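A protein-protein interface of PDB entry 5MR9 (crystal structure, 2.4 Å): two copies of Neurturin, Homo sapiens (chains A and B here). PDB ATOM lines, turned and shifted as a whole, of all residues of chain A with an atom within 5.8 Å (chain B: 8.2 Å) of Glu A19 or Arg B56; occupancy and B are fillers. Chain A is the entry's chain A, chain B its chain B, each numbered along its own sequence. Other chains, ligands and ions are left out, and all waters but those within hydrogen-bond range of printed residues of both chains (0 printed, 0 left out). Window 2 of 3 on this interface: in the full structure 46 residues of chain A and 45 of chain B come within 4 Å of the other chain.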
ATOM      1  N   VAL A  15      29.908  24.598  10.751  1.00  0.00           N
ATOM      2  CA  VAL A  15      29.264  24.126   9.514  1.00  0.00           C
ATOM      3  C   VAL A  15      29.389  25.156   8.398  1.00  0.00           C
ATOM      4  O   VAL A  15      29.490  26.350   8.678  1.00  0.00           O
ATOM      5  CB  VAL A  15      27.764  23.732   9.708  1.00  0.00           C
ATOM      6  CG1 VAL A  15      27.585  22.670  10.779  1.00  0.00           C
ATOM      7  CG2 VAL A  15      26.875  24.944   9.995  1.00  0.00           C
ATOM      8  N   ARG A  16      29.309  24.698   7.134  1.00  0.00           N
ATOM      9  CA  ARG A  16      29.244  25.577   5.967  1.00  0.00           C
ATOM     10  C   ARG A  16      27.764  25.919   5.902  1.00  0.00           C
ATOM     11  O   ARG A  16      26.946  25.061   6.246  1.00  0.00           O
ATOM     12  CB  ARG A  16      29.669  24.836   4.688  1.00  0.00           C
ATOM     13  CG  ARG A  16      31.168  24.648   4.547  1.00  0.00           C
ATOM     14  CD  ARG A  16      31.531  23.324   3.880  1.00  0.00           C
ATOM     15  NE  ARG A  16      31.856  23.444   2.456  1.00  0.00           N
ATOM     16  CZ  ARG A  16      32.996  23.934   1.972  1.00  0.00           C
ATOM     17  NH1 ARG A  16      33.926  24.409   2.799  1.00  0.00           N
ATOM     18  NH2 ARG A  16      33.205  23.987   0.665  1.00  0.00           N
ATOM     19  N   VAL A  17      27.399  27.157   5.523  1.00  0.00           N
ATOM     20  CA  VAL A  17      25.980  27.533   5.461  1.00  0.00           C
ATOM     21  C   VAL A  17      25.165  26.667   4.463  1.00  0.00           C
ATOM     22  O   VAL A  17      24.013  26.320   4.744  1.00  0.00           O
ATOM     23  CB  VAL A  17      25.738  29.066   5.378  1.00  0.00           C
ATOM     24  CG1 VAL A  17      26.028  29.623   3.993  1.00  0.00           C
ATOM     25  CG2 VAL A  17      24.332  29.437   5.839  1.00  0.00           C
ATOM     26  N   SER A  18      25.812  26.254   3.351  1.00  0.00           N
ATOM     27  CA  SER A  18      25.262  25.377   2.303  1.00  0.00           C
ATOM     28  C   SER A  18      24.886  23.984   2.834  1.00  0.00           C
ATOM     29  O   SER A  18      23.932  23.380   2.335  1.00  0.00           O
ATOM     30  CB  SER A  18      26.247  25.241   1.147  1.00  0.00           C
ATOM     31  OG  SER A  18      27.574  25.579   1.518  1.00  0.00           O
ATOM     32  N   GLU A  19      25.634  23.483   3.848  1.00  0.00           N
ATOM     33  CA  GLU A  19      25.400  22.180   4.488  1.00  0.00           C
ATOM     34  C   GLU A  19      24.098  22.161   5.300  1.00  0.00           C
ATOM     35  O   GLU A  19      23.602  21.079   5.601  1.00  0.00           O
ATOM     36  CB  GLU A  19      26.561  21.785   5.424  1.00  0.00           C
ATOM     37  CG  GLU A  19      27.925  21.582   4.776  1.00  0.00           C
ATOM     38  CD  GLU A  19      28.106  20.408   3.831  1.00  0.00           C
ATOM     39  OE1 GLU A  19      27.453  19.358   4.029  1.00  0.00           O
ATOM     40  OE2 GLU A  19      28.931  20.535   2.899  1.00  0.00           O
ATOM     41  N   LEU A  20      23.568  23.336   5.687  1.00  0.00           N
ATOM     42  CA  LEU A  20      22.350  23.444   6.503  1.00  0.00           C
ATOM     43  C   LEU A  20      21.048  23.127   5.764  1.00  0.00           C
ATOM     44  O   LEU A  20      20.020  22.896   6.411  1.00  0.00           O
ATOM     45  CB  LEU A  20      22.239  24.825   7.172  1.00  0.00           C
ATOM     46  CG  LEU A  20      23.245  25.176   8.272  1.00  0.00           C
ATOM     47  CD1 LEU A  20      23.105  26.630   8.668  1.00  0.00           C
ATOM     48  CD2 LEU A  20      23.070  24.297   9.504  1.00  0.00           C
ATOM     49  N   GLY A  21      21.086  23.157   4.435  1.00  0.00           N
ATOM     50  CA  GLY A  21      19.905  22.914   3.616  1.00  0.00           C
ATOM     51  C   GLY A  21      18.877  24.016   3.755  1.00  0.00           C
ATOM     52  O   GLY A  21      17.676  23.744   3.794  1.00  0.00           O
ATOM     53  N   LEU B  48      15.380  22.824  10.382  1.00  0.00           N
ATOM     54  CA  LEU B  48      15.791  22.531   9.003  1.00  0.00           C
ATOM     55  C   LEU B  48      17.275  22.201   8.952  1.00  0.00           C
ATOM     56  O   LEU B  48      17.668  21.241   8.285  1.00  0.00           O
ATOM     57  CB  LEU B  48      15.527  23.766   8.134  1.00  0.00           C
ATOM     58  CG  LEU B  48      14.538  23.700   6.978  1.00  0.00           C
ATOM     59  CD1 LEU B  48      13.540  22.539   7.106  1.00  0.00           C
ATOM     60  CD2 LEU B  48      13.833  25.024   6.855  1.00  0.00           C
ATOM     61  N   GLY B  49      18.079  23.018   9.641  1.00  0.00           N
ATOM     62  CA  GLY B  49      19.522  22.849   9.728  1.00  0.00           C
ATOM     63  C   GLY B  49      19.910  21.624  10.531  1.00  0.00           C
ATOM     64  O   GLY B  49      20.820  20.899  10.141  1.00  0.00           O
ATOM     65  N   LEU B  50      19.194  21.370  11.639  1.00  0.00           N
ATOM     66  CA  LEU B  50      19.415  20.234  12.529  1.00  0.00           C
ATOM     67  C   LEU B  50      19.091  18.909  11.844  1.00  0.00           C
ATOM     68  O   LEU B  50      19.861  17.959  11.985  1.00  0.00           O
ATOM     69  CB  LEU B  50      18.613  20.396  13.836  1.00  0.00           C
ATOM     70  CG  LEU B  50      19.059  19.569  15.049  1.00  0.00           C
ATOM     71  CD1 LEU B  50      20.543  19.774  15.372  1.00  0.00           C
ATOM     72  CD2 LEU B  50      18.212  19.887  16.260  1.00  0.00           C
ATOM     73  N   ARG B  51      17.957  18.846  11.105  1.00  0.00           N
ATOM     74  CA  ARG B  51      17.540  17.648  10.361  1.00  0.00           C
ATOM     75  C   ARG B  51      18.531  17.318   9.263  1.00  0.00           C
ATOM     76  O   ARG B  51      18.870  16.149   9.077  1.00  0.00           O
ATOM     77  CB  ARG B  51      16.133  17.810   9.772  1.00  0.00           C
ATOM     78  CG  ARG B  51      15.037  17.416  10.739  1.00  0.00           C
ATOM     79  CD  ARG B  51      13.679  17.231  10.076  1.00  0.00           C
ATOM     80  NE  ARG B  51      13.050  18.492   9.675  1.00  0.00           N
ATOM     81  CZ  ARG B  51      12.410  19.323  10.493  1.00  0.00           C
ATOM     82  NH1 ARG B  51      11.863  20.435  10.033  1.00  0.00           N
ATOM     83  NH2 ARG B  51      12.319  19.041  11.790  1.00  0.00           N
ATOM     84  N   ARG B  52      19.022  18.354   8.564  1.00  0.00           N
ATOM     85  CA  ARG B  52      19.995  18.213   7.488  1.00  0.00           C
ATOM     86  C   ARG B  52      21.346  17.711   7.991  1.00  0.00           C
ATOM     87  O   ARG B  52      21.970  16.887   7.322  1.00  0.00           O
ATOM     88  CB  ARG B  52      20.124  19.531   6.706  1.00  0.00           C
ATOM     89  CG  ARG B  52      20.921  19.440   5.406  1.00  0.00           C
ATOM     90  CD  ARG B  52      20.302  18.545   4.342  1.00  0.00           C
ATOM     91  NE  ARG B  52      19.705  19.313   3.249  1.00  0.00           N
ATOM     92  CZ  ARG B  52      20.370  19.751   2.183  1.00  0.00           C
ATOM     93  NH1 ARG B  52      21.674  19.535   2.069  1.00  0.00           N
ATOM     94  NH2 ARG B  52      19.742  20.435   1.237  1.00  0.00           N
ATOM     95  N   LEU B  53      21.784  18.176   9.177  1.00  0.00           N
ATOM     96  CA  LEU B  53      23.057  17.753   9.774  1.00  0.00           C
ATOM     97  C   LEU B  53      23.004  16.313  10.298  1.00  0.00           C
ATOM     98  O   LEU B  53      24.034  15.641  10.379  1.00  0.00           O
ATOM     99  CB  LEU B  53      23.494  18.715  10.887  1.00  0.00           C
ATOM    100  CG  LEU B  53      23.999  20.079  10.438  1.00  0.00           C
ATOM    101  CD1 LEU B  53      23.986  21.049  11.583  1.00  0.00           C
ATOM    102  CD2 LEU B  53      25.373  19.980   9.809  1.00  0.00           C
ATOM    103  N   ARG B  54      21.798  15.857  10.650  1.00  0.00           N
ATOM    104  CA  ARG B  54      21.511  14.511  11.130  1.00  0.00           C
ATOM    105  C   ARG B  54      21.629  13.520   9.963  1.00  0.00           C
ATOM    106  O   ARG B  54      22.097  12.399  10.161  1.00  0.00           O
ATOM    107  CB  ARG B  54      20.097  14.491  11.702  1.00  0.00           C
ATOM    108  CG  ARG B  54      19.851  13.456  12.770  1.00  0.00           C
ATOM    109  CD  ARG B  54      18.478  13.708  13.350  1.00  0.00           C
ATOM    110  NE  ARG B  54      17.595  12.556  13.217  1.00  0.00           N
ATOM    111  CZ  ARG B  54      16.277  12.637  13.068  1.00  0.00           C
ATOM    112  NH1 ARG B  54      15.678  13.822  13.013  1.00  0.00           N
ATOM    113  NH2 ARG B  54      15.548  11.535  12.956  1.00  0.00           N
ATOM    114  N   GLN B  55      21.212  13.953   8.747  1.00  0.00           N
ATOM    115  CA  GLN B  55      21.277  13.184   7.496  1.00  0.00           C
ATOM    116  C   GLN B  55      22.729  12.936   7.087  1.00  0.00           C
ATOM    117  O   GLN B  55      23.044  11.868   6.564  1.00  0.00           O
ATOM    118  CB  GLN B  55      20.534  13.916   6.361  1.00  0.00           C
ATOM    119  CG  GLN B  55      19.004  13.934   6.498  1.00  0.00           C
ATOM    120  CD  GLN B  55      18.315  14.836   5.487  1.00  0.00           C
ATOM    121  OE1 GLN B  55      18.689  14.911   4.309  1.00  0.00           O
ATOM    122  NE2 GLN B  55      17.256  15.508   5.916  1.00  0.00           N
ATOM    123  N   ARG B  56      23.612  13.913   7.351  1.00  0.00           N
ATOM    124  CA  ARG B  56      25.047  13.860   7.062  1.00  0.00           C
ATOM    125  C   ARG B  56      25.823  13.068   8.131  1.00  0.00           C
ATOM    126  O   ARG B  56      27.022  12.828   7.954  1.00  0.00           O
ATOM    127  CB  ARG B  56      25.627  15.287   6.967  1.00  0.00           C
ATOM    128  CG  ARG B  56      24.956  16.221   5.967  1.00  0.00           C
ATOM    129  CD  ARG B  56      25.632  16.200   4.612  1.00  0.00           C
ATOM    130  NE  ARG B  56      25.488  17.484   3.930  1.00  0.00           N
ATOM    131  CZ  ARG B  56      24.465  17.824   3.152  1.00  0.00           C
ATOM    132  NH1 ARG B  56      23.475  16.964   2.932  1.00  0.00           N
ATOM    133  NH2 ARG B  56      24.429  19.017   2.578  1.00  0.00           N
ATOM    134  N   ARG B  57      25.145  12.683   9.247  1.00  0.00           N
ATOM    135  CA  ARG B  57      25.691  11.947  10.410  1.00  0.00           C
ATOM    136  C   ARG B  57      26.794  12.755  11.115  1.00  0.00           C
ATOM    137  O   ARG B  57      27.808  12.201  11.558  1.00  0.00           O
ATOM    138  CB  ARG B  57      26.177  10.526  10.029  1.00  0.00           C
ATOM    139  CG  ARG B  57      25.135   9.663   9.336  1.00  0.00           C
ATOM    140  CD  ARG B  57      24.360   8.796  10.305  1.00  0.00           C
ATOM    141  NE  ARG B  57      23.086   8.380   9.720  1.00  0.00           N
ATOM    142  CZ  ARG B  57      21.897   8.815  10.122  1.00  0.00           C
ATOM    143  NH1 ARG B  57      21.801   9.661  11.142  1.00  0.00           N
ATOM    144  NH2 ARG B  57      20.791   8.392   9.523  1.00  0.00           N
ATOM    145  N   ARG B  58      26.565  14.075  11.230  1.00  0.00           N
ATOM    146  CA  ARG B  58      27.499  15.034  11.817  1.00  0.00           C
ATOM    147  C   ARG B  58      27.159  15.442  13.260  1.00  0.00           C
ATOM    148  O   ARG B  58      27.811  16.333  13.814  1.00  0.00           O
ATOM    149  CB  ARG B  58      27.569  16.272  10.918  1.00  0.00           C
ATOM    150  CG  ARG B  58      28.052  15.974   9.507  1.00  0.00           C
ATOM    151  CD  ARG B  58      28.531  17.233   8.830  1.00  0.00           C
ATOM    152  NE  ARG B  58      29.635  17.814   9.588  1.00  0.00           N
ATOM    153  CZ  ARG B  58      29.950  19.101   9.602  1.00  0.00           C
ATOM    154  NH1 ARG B  58      29.259  19.967   8.870  1.00  0.00           N
ATOM    155  NH2 ARG B  58      30.961  19.535  10.339  1.00  0.00           N
ATOM    156  N   LEU B  59      26.169  14.770  13.874  1.00  0.00           N
ATOM    157  CA  LEU B  59      25.653  15.089  15.205  1.00  0.00           C
ATOM    158  C   LEU B  59      26.156  14.247  16.401  1.00  0.00           C
ATOM    159  O   LEU B  59      25.517  14.255  17.458  1.00  0.00           O
ATOM    160  CB  LEU B  59      24.109  15.201  15.166  1.00  0.00           C
ATOM    161  CG  LEU B  59      23.497  16.263  14.213  1.00  0.00           C
ATOM    162  CD1 LEU B  59      21.999  16.361  14.399  1.00  0.00           C
ATOM    163  CD2 LEU B  59      24.117  17.642  14.418  1.00  0.00           C
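OE1 of Glu A19 is in salt-bridge range of NE of Arg B56. O of Leu A20 lies close to O of Leu B48 (3.4 Å).
The backbone NH (N) of Arg B58 lies within hydrogen-bond range of the backbone carbonyl oxygen (O) of Leu B53 (3.1 Å).
Among the printed residues, merely in contact across the chains: Val A15 with Leu B53 (3.6 Å), Val A15 with Arg B58 (3.7 Å), Glu A19 with Arg B52 (3.1 Å), Leu A20 with Gly B49 (3.4 Å), Leu A20 with Arg B52 (3.4 Å), Leu A20 with Leu B53 (3.96 Å) and Gly A21 with Arg B52 (3.4 Å).
Of chain B, only Arg B52 (3.1 Å) and Arg B56 (2.7 Å) come within 4 Å of Glu A19. Of the printed residues of chain A, Arg B58 touches Val A15. Of the printed residues of chain A, Arg B52 touches Glu A19, Leu A20 and Gly A21. Of the printed residues of chain A, Leu B48 touches Leu A20 (3.4 Å). Of the printed residues of chain B, Leu A20 touches Leu B48, Gly B49, Arg B52 and Leu B53. Of the printed residues of chain B, Gly A21 touches Arg B52. Arg B51 touches none of the printed residues of chain A. Arg B57 touches none of the printed residues of chain A. The nearest residue of chain B that does not touch Glu A19 is Arg B58 (4.6 Å).
Hydrophobic or aromatic side chains of chain B within 4 Å of the printed part of chain A: Leu B53. Of the 7 printed residues of chain A, 4 touch a printed residue of chain B. Hydrophobic or aromatic side chains of chain A within 4 Å of the printed part of chain B: Val A15 and Leu A20. Among the printed residues, 9 pairs touch across the chains.
No position is printed for both chains. Of the 9 pairs that touch across the chains among the printed residues, none has its exchanged pair printed and touching as well.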
